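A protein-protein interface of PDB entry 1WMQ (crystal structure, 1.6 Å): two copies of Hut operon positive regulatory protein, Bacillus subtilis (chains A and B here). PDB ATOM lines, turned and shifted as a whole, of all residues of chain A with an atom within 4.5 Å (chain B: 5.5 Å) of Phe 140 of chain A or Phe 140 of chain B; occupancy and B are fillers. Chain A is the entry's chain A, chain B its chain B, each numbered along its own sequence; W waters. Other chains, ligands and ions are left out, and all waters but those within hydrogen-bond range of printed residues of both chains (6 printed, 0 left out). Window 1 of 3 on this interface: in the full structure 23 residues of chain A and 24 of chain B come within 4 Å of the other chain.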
ATOM      1  N   GLY A   9     -11.530 -11.740 -14.033  1.00  0.00           N
ATOM      2  CA  GLY A   9     -10.527 -11.142 -13.167  1.00  0.00           C
ATOM      3  C   GLY A   9     -10.583  -9.626 -13.211  1.00  0.00           C
ATOM      4  O   GLY A   9     -10.726  -8.963 -12.179  1.00  0.00           O
ATOM      5  N   ARG A  10     -10.471  -9.084 -14.417  1.00  0.00           N
ATOM      6  CA  ARG A  10     -10.515  -7.641 -14.628  1.00  0.00           C
ATOM      7  C   ARG A  10     -11.813  -7.038 -14.092  1.00  0.00           C
ATOM      8  O   ARG A  10     -11.796  -6.009 -13.417  1.00  0.00           O
ATOM      9  CB  ARG A  10     -10.371  -7.338 -16.121  1.00  0.00           C
ATOM     10  CG  ARG A  10     -10.502  -5.872 -16.487  1.00  0.00           C
ATOM     11  CD  ARG A  10     -10.104  -5.648 -17.942  1.00  0.00           C
ATOM     12  NE  ARG A  10     -10.267  -4.257 -18.355  1.00  0.00           N
ATOM     13  CZ  ARG A  10     -11.438  -3.683 -18.611  1.00  0.00           C
ATOM     14  NH1 ARG A  10     -12.562  -4.381 -18.504  1.00  0.00           N
ATOM     15  NH2 ARG A  10     -11.486  -2.408 -18.971  1.00  0.00           N
ATOM     16  N   VAL A  13     -11.893  -6.819 -10.305  1.00  0.00           N
ATOM     17  CA  VAL A  13     -10.978  -5.788  -9.831  1.00  0.00           C
ATOM     18  C   VAL A  13     -11.563  -4.394 -10.032  1.00  0.00           C
ATOM     19  O   VAL A  13     -11.463  -3.547  -9.147  1.00  0.00           O
ATOM     20  CB  VAL A  13      -9.610  -5.889 -10.552  1.00  0.00           C
ATOM     21  CG1 VAL A  13      -8.722  -4.710 -10.170  1.00  0.00           C
ATOM     22  CG2 VAL A  13      -8.924  -7.202 -10.174  1.00  0.00           C
ATOM     23  N   GLY A  84      -0.917 -12.627  -3.357  1.00  0.00           N
ATOM     24  CA  GLY A  84      -0.639 -11.284  -3.827  1.00  0.00           C
ATOM     25  C   GLY A  84      -0.603 -10.313  -2.669  1.00  0.00           C
ATOM     26  O   GLY A  84       0.153  -9.345  -2.672  1.00  0.00           O
ATOM     27  N   VAL A  85      -1.426 -10.585  -1.663  1.00  0.00           N
ATOM     28  CA  VAL A  85      -1.496  -9.731  -0.496  1.00  0.00           C
ATOM     29  C   VAL A  85      -0.317  -9.912   0.446  1.00  0.00           C
ATOM     30  O   VAL A  85       0.244  -8.925   0.919  1.00  0.00           O
ATOM     31  CB  VAL A  85      -2.819  -9.975   0.278  1.00  0.00           C
ATOM     32  CG1 VAL A  85      -2.780  -9.290   1.638  1.00  0.00           C
ATOM     33  CG2 VAL A  85      -3.997  -9.448  -0.542  1.00  0.00           C
ATOM     34  N   LEU A 124      -8.828  -8.906  -3.836  1.00  0.00           N
ATOM     35  CA  LEU A 124      -8.598  -8.204  -2.584  1.00  0.00           C
ATOM     36  C   LEU A 124      -7.829  -6.913  -2.797  1.00  0.00           C
ATOM     37  O   LEU A 124      -6.869  -6.878  -3.565  1.00  0.00           O
ATOM     38  CB  LEU A 124      -7.789  -9.097  -1.644  1.00  0.00           C
ATOM     39  CG  LEU A 124      -8.254 -10.545  -1.485  1.00  0.00           C
ATOM     40  CD1 LEU A 124      -7.248 -11.316  -0.644  1.00  0.00           C
ATOM     41  CD2 LEU A 124      -9.627 -10.578  -0.835  1.00  0.00           C
ATOM     42  N   TYR A 125      -8.264  -5.854  -2.115  1.00  0.00           N
ATOM     43  CA  TYR A 125      -7.586  -4.563  -2.185  1.00  0.00           C
ATOM     44  C   TYR A 125      -7.709  -3.827  -0.864  1.00  0.00           C
ATOM     45  O   TYR A 125      -8.788  -3.761  -0.274  1.00  0.00           O
ATOM     46  CB  TYR A 125      -8.151  -3.671  -3.289  1.00  0.00           C
ATOM     47  CG  TYR A 125      -7.604  -2.263  -3.197  1.00  0.00           C
ATOM     48  CD1 TYR A 125      -6.258  -2.002  -3.447  1.00  0.00           C
ATOM     49  CD2 TYR A 125      -8.413  -1.200  -2.791  1.00  0.00           C
ATOM     50  CE1 TYR A 125      -5.724  -0.720  -3.291  1.00  0.00           C
ATOM     51  CE2 TYR A 125      -7.892   0.088  -2.632  1.00  0.00           C
ATOM     52  CZ  TYR A 125      -6.546   0.320  -2.882  1.00  0.00           C
ATOM     53  OH  TYR A 125      -6.018   1.580  -2.710  1.00  0.00           O
ATOM     54  N   THR A 139      -2.127  -2.989  -0.830  1.00  0.00           N
ATOM     55  CA  THR A 139      -1.876  -4.392  -1.103  1.00  0.00           C
ATOM     56  C   THR A 139      -2.990  -4.871  -2.023  1.00  0.00           C
ATOM     57  O   THR A 139      -4.117  -4.353  -1.976  1.00  0.00           O
ATOM     58  CB  THR A 139      -1.815  -5.218   0.191  1.00  0.00           C
ATOM     59  OG1 THR A 139      -1.339  -6.531  -0.121  1.00  0.00           O
ATOM     60  CG2 THR A 139      -3.189  -5.291   0.855  1.00  0.00           C
ATOM     61  N   PHE A 140      -2.671  -5.864  -2.849  1.00  0.00           N
ATOM     62  CA  PHE A 140      -3.589  -6.372  -3.853  1.00  0.00           C
ATOM     63  C   PHE A 140      -3.443  -7.884  -4.051  1.00  0.00           C
ATOM     64  O   PHE A 140      -2.360  -8.446  -3.859  1.00  0.00           O
ATOM     65  CB  PHE A 140      -3.268  -5.653  -5.164  1.00  0.00           C
ATOM     66  CG  PHE A 140      -4.368  -5.671  -6.165  1.00  0.00           C
ATOM     67  CD1 PHE A 140      -5.456  -4.813  -6.037  1.00  0.00           C
ATOM     68  CD2 PHE A 140      -4.305  -6.519  -7.265  1.00  0.00           C
ATOM     69  CE1 PHE A 140      -6.467  -4.797  -6.993  1.00  0.00           C
ATOM     70  CE2 PHE A 140      -5.313  -6.513  -8.228  1.00  0.00           C
ATOM     71  CZ  PHE A 140      -6.396  -5.646  -8.089  1.00  0.00           C
ATOM     72  N   GLY A 141      -4.533  -8.539  -4.444  1.00  0.00           N
ATOM     73  CA  GLY A 141      -4.484  -9.970  -4.678  1.00  0.00           C
ATOM     74  C   GLY A 141      -5.675 -10.482  -5.464  1.00  0.00           C
ATOM     75  O   GLY A 141      -6.811 -10.089  -5.210  1.00  0.00           O
ATOM     76  N   VAL A 142      -5.408 -11.338  -6.443  1.00  0.00           N
ATOM     77  CA  VAL A 142      -6.461 -11.934  -7.252  1.00  0.00           C
ATOM     78  C   VAL A 142      -6.196 -13.423  -7.425  1.00  0.00           C
ATOM     79  O   VAL A 142      -5.085 -13.831  -7.776  1.00  0.00           O
ATOM     80  CB  VAL A 142      -6.547 -11.284  -8.649  1.00  0.00           C
ATOM     81  CG1 VAL A 142      -7.666 -11.947  -9.469  1.00  0.00           C
ATOM     82  CG2 VAL A 142      -6.810  -9.792  -8.506  1.00  0.00           C
ATOM     83  N   VAL B  13      -3.103   0.410 -11.109  1.00  0.00           N
ATOM     84  CA  VAL B  13      -3.970  -0.683 -11.547  1.00  0.00           C
ATOM     85  C   VAL B  13      -5.030  -0.177 -12.527  1.00  0.00           C
ATOM     86  O   VAL B  13      -5.262  -0.786 -13.572  1.00  0.00           O
ATOM     87  CB  VAL B  13      -4.683  -1.343 -10.334  1.00  0.00           C
ATOM     88  CG1 VAL B  13      -5.679  -2.386 -10.810  1.00  0.00           C
ATOM     89  N   LEU B  17      -5.760  -1.362 -16.258  1.00  0.00           N
ATOM     90  CA  LEU B  17      -7.031  -1.997 -16.641  1.00  0.00           C
ATOM     91  C   LEU B  17      -7.966  -1.201 -17.553  1.00  0.00           C
ATOM     92  O   LEU B  17      -9.081  -1.642 -17.839  1.00  0.00           O
ATOM     93  CB  LEU B  17      -7.777  -2.436 -15.376  1.00  0.00           C
ATOM     94  CG  LEU B  17      -7.053  -3.536 -14.590  1.00  0.00           C
ATOM     95  CD1 LEU B  17      -7.908  -3.933 -13.406  1.00  0.00           C
ATOM     96  CD2 LEU B  17      -6.788  -4.745 -15.485  1.00  0.00           C
ATOM     97  N   ALA B  81       5.398  -7.933  -7.092  1.00  0.00           N
ATOM     98  CA  ALA B  81       4.301  -8.030  -8.047  1.00  0.00           C
ATOM     99  C   ALA B  81       4.269  -9.442  -8.629  1.00  0.00           C
ATOM    100  O   ALA B  81       3.194  -9.995  -8.887  1.00  0.00           O
ATOM    101  CB  ALA B  81       4.477  -6.995  -9.167  1.00  0.00           C
ATOM    102  N   GLY B  84       2.094 -12.146  -6.934  1.00  0.00           N
ATOM    103  CA  GLY B  84       0.682 -12.177  -7.247  1.00  0.00           C
ATOM    104  C   GLY B  84       0.431 -12.933  -8.528  1.00  0.00           C
ATOM    105  O   GLY B  84      -0.587 -13.611  -8.680  1.00  0.00           O
ATOM    106  N   VAL B  85       1.375 -12.819  -9.455  1.00  0.00           N
ATOM    107  CA  VAL B  85       1.254 -13.485 -10.732  1.00  0.00           C
ATOM    108  C   VAL B  85       1.553 -14.978 -10.658  1.00  0.00           C
ATOM    109  O   VAL B  85       0.830 -15.775 -11.247  1.00  0.00           O
ATOM    110  CB  VAL B  85       2.202 -12.846 -11.779  1.00  0.00           C
ATOM    111  CG1 VAL B  85       2.254 -13.701 -13.031  1.00  0.00           C
ATOM    112  CG2 VAL B  85       1.723 -11.438 -12.125  1.00  0.00           C
ATOM    113  N   LEU B 124       1.014  -5.604 -12.648  1.00  0.00           N
ATOM    114  CA  LEU B 124       0.988  -6.538 -13.760  1.00  0.00           C
ATOM    115  C   LEU B 124      -0.401  -7.115 -13.964  1.00  0.00           C
ATOM    116  O   LEU B 124      -1.091  -7.443 -12.998  1.00  0.00           O
ATOM    117  CB  LEU B 124       1.954  -7.691 -13.479  1.00  0.00           C
ATOM    118  CG  LEU B 124       3.357  -7.318 -12.999  1.00  0.00           C
ATOM    119  CD1 LEU B 124       4.112  -8.574 -12.609  1.00  0.00           C
ATOM    120  CD2 LEU B 124       4.101  -6.580 -14.103  1.00  0.00           C
ATOM    121  N   TYR B 125      -0.804  -7.236 -15.227  1.00  0.00           N
ATOM    122  CA  TYR B 125      -2.092  -7.825 -15.573  1.00  0.00           C
ATOM    123  C   TYR B 125      -2.009  -8.528 -16.918  1.00  0.00           C
ATOM    124  O   TYR B 125      -1.444  -7.999 -17.878  1.00  0.00           O
ATOM    125  CB  TYR B 125      -3.217  -6.785 -15.628  1.00  0.00           C
ATOM    126  CG  TYR B 125      -4.493  -7.368 -16.205  1.00  0.00           C
ATOM    127  CD1 TYR B 125      -5.198  -8.362 -15.525  1.00  0.00           C
ATOM    128  CD2 TYR B 125      -4.951  -6.990 -17.466  1.00  0.00           C
ATOM    129  CE1 TYR B 125      -6.322  -8.973 -16.087  1.00  0.00           C
ATOM    130  CE2 TYR B 125      -6.077  -7.595 -18.040  1.00  0.00           C
ATOM    131  CZ  TYR B 125      -6.754  -8.588 -17.345  1.00  0.00           C
ATOM    132  OH  TYR B 125      -7.844  -9.214 -17.914  1.00  0.00           O
ATOM    133  N   GLY B 126      -2.582  -9.722 -16.985  1.00  0.00           N
ATOM    134  CA  GLY B 126      -2.564 -10.470 -18.224  1.00  0.00           C
ATOM    135  C   GLY B 126      -3.106 -11.861 -18.020  1.00  0.00           C
ATOM    136  O   GLY B 126      -4.037 -12.069 -17.237  1.00  0.00           O
ATOM    137  N   GLU B 138      -6.740 -15.275 -16.281  1.00  0.00           N
ATOM    138  CA  GLU B 138      -6.121 -14.015 -15.908  1.00  0.00           C
ATOM    139  C   GLU B 138      -5.183 -14.120 -14.718  1.00  0.00           C
ATOM    140  O   GLU B 138      -5.259 -15.050 -13.915  1.00  0.00           O
ATOM    141  CB  GLU B 138      -7.199 -12.978 -15.597  1.00  0.00           C
ATOM    142  CG  GLU B 138      -7.992 -12.531 -16.804  1.00  0.00           C
ATOM    143  CD  GLU B 138      -9.313 -11.922 -16.415  1.00  0.00           C
ATOM    144  OE1 GLU B 138     -10.248 -12.691 -16.102  1.00  0.00           O
ATOM    145  OE2 GLU B 138      -9.410 -10.680 -16.398  1.00  0.00           O
ATOM    146  N   THR B 139      -4.286 -13.153 -14.621  1.00  0.00           N
ATOM    147  CA  THR B 139      -3.347 -13.094 -13.516  1.00  0.00           C
ATOM    148  C   THR B 139      -3.076 -11.613 -13.225  1.00  0.00           C
ATOM    149  O   THR B 139      -3.125 -10.778 -14.136  1.00  0.00           O
ATOM    150  CB  THR B 139      -2.047 -13.869 -13.856  1.00  0.00           C
ATOM    151  OG1 THR B 139      -1.225 -13.962 -12.686  1.00  0.00           O
ATOM    152  CG2 THR B 139      -1.273 -13.182 -14.982  1.00  0.00           C
ATOM    153  N   PHE B 140      -2.829 -11.297 -11.954  1.00  0.00           N
ATOM    154  CA  PHE B 140      -2.569  -9.931 -11.493  1.00  0.00           C
ATOM    155  C   PHE B 140      -1.452  -9.922 -10.458  1.00  0.00           C
ATOM    156  O   PHE B 140      -1.250 -10.899  -9.727  1.00  0.00           O
ATOM    157  CB  PHE B 140      -3.767  -9.311 -10.760  1.00  0.00           C
ATOM    158  CG  PHE B 140      -4.946  -8.985 -11.617  1.00  0.00           C
ATOM    159  CD1 PHE B 140      -5.788  -9.986 -12.094  1.00  0.00           C
ATOM    160  CD2 PHE B 140      -5.283  -7.652 -11.854  1.00  0.00           C
ATOM    161  CE1 PHE B 140      -6.962  -9.664 -12.781  1.00  0.00           C
ATOM    162  CE2 PHE B 140      -6.451  -7.318 -12.540  1.00  0.00           C
ATOM    163  CZ  PHE B 140      -7.293  -8.325 -13.003  1.00  0.00           C
ATOM    164  N   GLY B 141      -0.776  -8.786 -10.353  1.00  0.00           N
ATOM    165  CA  GLY B 141       0.280  -8.658  -9.370  1.00  0.00           C
ATOM    166  C   GLY B 141       0.623  -7.204  -9.123  1.00  0.00           C
ATOM    167  O   GLY B 141       0.729  -6.423 -10.062  1.00  0.00           O
ATOM    168  N   VAL B 142       0.769  -6.829  -7.857  1.00  0.00           N
ATOM    169  CA  VAL B 142       1.136  -5.467  -7.514  1.00  0.00           C
ATOM    170  C   VAL B 142       2.193  -5.488  -6.421  1.00  0.00           C
ATOM    171  O   VAL B 142       2.027  -6.153  -5.395  1.00  0.00           O
ATOM    172  CB  VAL B 142      -0.080  -4.646  -7.018  1.00  0.00           C
ATOM    173  CG1 VAL B 142       0.357  -3.220  -6.629  1.00  0.00           C
ATOM    174  CG2 VAL B 142      -1.133  -4.591  -8.108  1.00  0.00           C
HETATM  175  O   HOH W   1       1.737  -9.306  -5.446  1.00  0.00           O
HETATM  176  O   HOH W   2      -0.874  -8.690  -6.159  1.00  0.00           O
HETATM  177  O   HOH W   3      -3.181 -13.598  -9.884  1.00  0.00           O
HETATM  178  O   HOH W   4      -2.405 -13.439  -6.168  1.00  0.00           O
HETATM  179  O   HOH W   5       0.270  -6.557  -3.240  1.00  0.00           O
HETATM  180  O   HOH W   6      -2.538 -10.891  -7.312  1.00  0.00           O
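Of the printed residues of chain B, Arg 10 of chain A touches Leu 17 (2.8 Å), Tyr 125 (3.6 Å), Glu 138 (2.8 Å) and Phe 140 (3.6 Å).
Printed residues of chain B within 4 Å of Val 13 of chain A: Val 13 (3.9 Å), Leu 17 (3.4 Å) and Phe 140 (3.4 Å).
Phe 140 of chain A touches just these residues of chain B: Phe 140 (3.8 Å) and Val 142 (3.8 Å).
Gly 141 of chain A touches none of the printed residues of chain B.
Printed residues of chain B within 4 Å of Val 142 of chain A: Phe 140 (3.7 Å).
Of the printed residues of chain A, Val 13 of chain B touches Val 13.
Of the printed residues of chain A, Tyr 125 of chain B touches Arg 10.
Of chain A, only Gly 9, Arg 10, Val 13, Phe 140 and Val 142 come within 4 Å of Phe 140 of chain B.
Gly 141 of chain B touches none of the printed residues of chain A.
The nearest printed residue of chain B that does not touch Val 142 of chain A is Gly 84 of chain B (4.6 Å).
Of the 13 printed residues of chain B, 7 touch a printed residue of chain A.
Hydrophobic or aromatic side chains of chain B that line the printed part of chain A: Val 13, Leu 17, Tyr 125, Phe 140 and Val 142.
Printed residues of chain A that touch a printed residue of chain B: Gly 9, Arg 10, Val 13, Gly 84, Phe 140 and Val 142.
Hydrophobic or aromatic side chains of chain A that line the printed part of chain B: Val 13, Phe 140 and Val 142.
Among the printed residues, no Asp or Glu carboxylate lies within 4 Å of a Lys or Arg side-chain nitrogen of the other chain.
OE2 of Glu 138 of chain B lies within hydrogen-bond range of OH of Tyr 125 of chain B, at 2.6 Å.
The backbone carbonyl oxygen (O) of Phe 140 of chain B lies within hydrogen-bond range of the backbone NH (N) of Val 85 of chain B (3.3 Å).
The backbone NH of Val 85 of chain A is in hydrogen-bond range of the backbone carbonyl oxygen of Phe 140 of chain A, at 3.2 Å.
Val 13 of chain B touches its own counterpart, Val 13 of chain A.
Gly 84 of chain B touches its own counterpart, Gly 84 of chain A.
Phe 140 of chain B touches its own counterpart, Phe 140 of chain A.
Phe 140 of chain A touches Val 142 of chain B, and with the chains exchanged Val 142 of chain A touches Phe 140 of chain B.
9 positions are printed for both chains.
Of the 13 pairs that touch across the chains among the printed residues, 5 have their exchanged pair printed and touching as well.
The backbone NH (N) of Gly 9 of chain A lies within hydrogen-bond range of the side-chain carboxylate (OE1) of Glu 138 of chain B (2.6 Å).
O of Leu 17 of chain B sits at hydrogen-bond distance from NH2 of Arg 10 of chain A (2.8 Å).
The backbone NH of Arg 10 of chain A is in hydrogen-bond range of the side-chain carboxylate of Glu 138 of chain B (2.8 Å).
Water W6 bridges O of Phe 140 of chain B (2.7 Å) and N of Val 142 of chain A (3.0 Å).
Water W2 lies within hydrogen-bond range of the backbone carbonyl oxygen of Phe 140 of chain A (2.7 Å) and the backbone NH of Val 142 of chain B (3.0 Å).
Water W5 lies within hydrogen-bond range of the backbone carbonyl oxygen of Val 142 of chain B (2.8 Å), the backbone carbonyl oxygen of Gly 84 of chain A (2.8 Å) and the backbone NH of Phe 140 of chain A (3.0 Å).
Water W3 lies within hydrogen-bond range of the backbone carbonyl oxygen of Val 142 of chain A, the backbone carbonyl oxygen of Gly 84 of chain B, the backbone NH of Phe 140 of chain B and the side-chain hydroxyl of Thr 139 of chain B.
Water W4 lies within hydrogen-bond range of the backbone carbonyl oxygen of Gly 84 of chain B (3.1 Å), the backbone carbonyl oxygen of Val 142 of chain A (3.1 Å) and the backbone NH of Gly 84 of chain A (3.3 Å).
Water W1 lies within hydrogen-bond range of O of Val 142 of chain B, O of Gly 84 of chain A and N of Gly 84 of chain B.
Among the printed residues, pairs that only touch across the chains: Val 13 of chain A with Phe 140 of chain B (3.4 Å), Val 13 of chain A with Leu 17 of chain B (3.4 Å), Gly 9 of chain A with Phe 140 of chain B (3.5 Å), Arg 10 of chain A with Phe 140 of chain B (3.6 Å), Arg 10 of chain A with Tyr 125 of chain B (3.6 Å), Val 142 of chain A with Phe 140 of chain B (3.7 Å), Gly 84 of chain A with Gly 84 of chain B (3.8 Å), Phe 140 of chain A with Val 142 of chain B (3.8 Å), Phe 140 of chain A with Phe 140 of chain B (3.8 Å) and Val 13 of chain A with Val 13 of chain B (3.9 Å).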
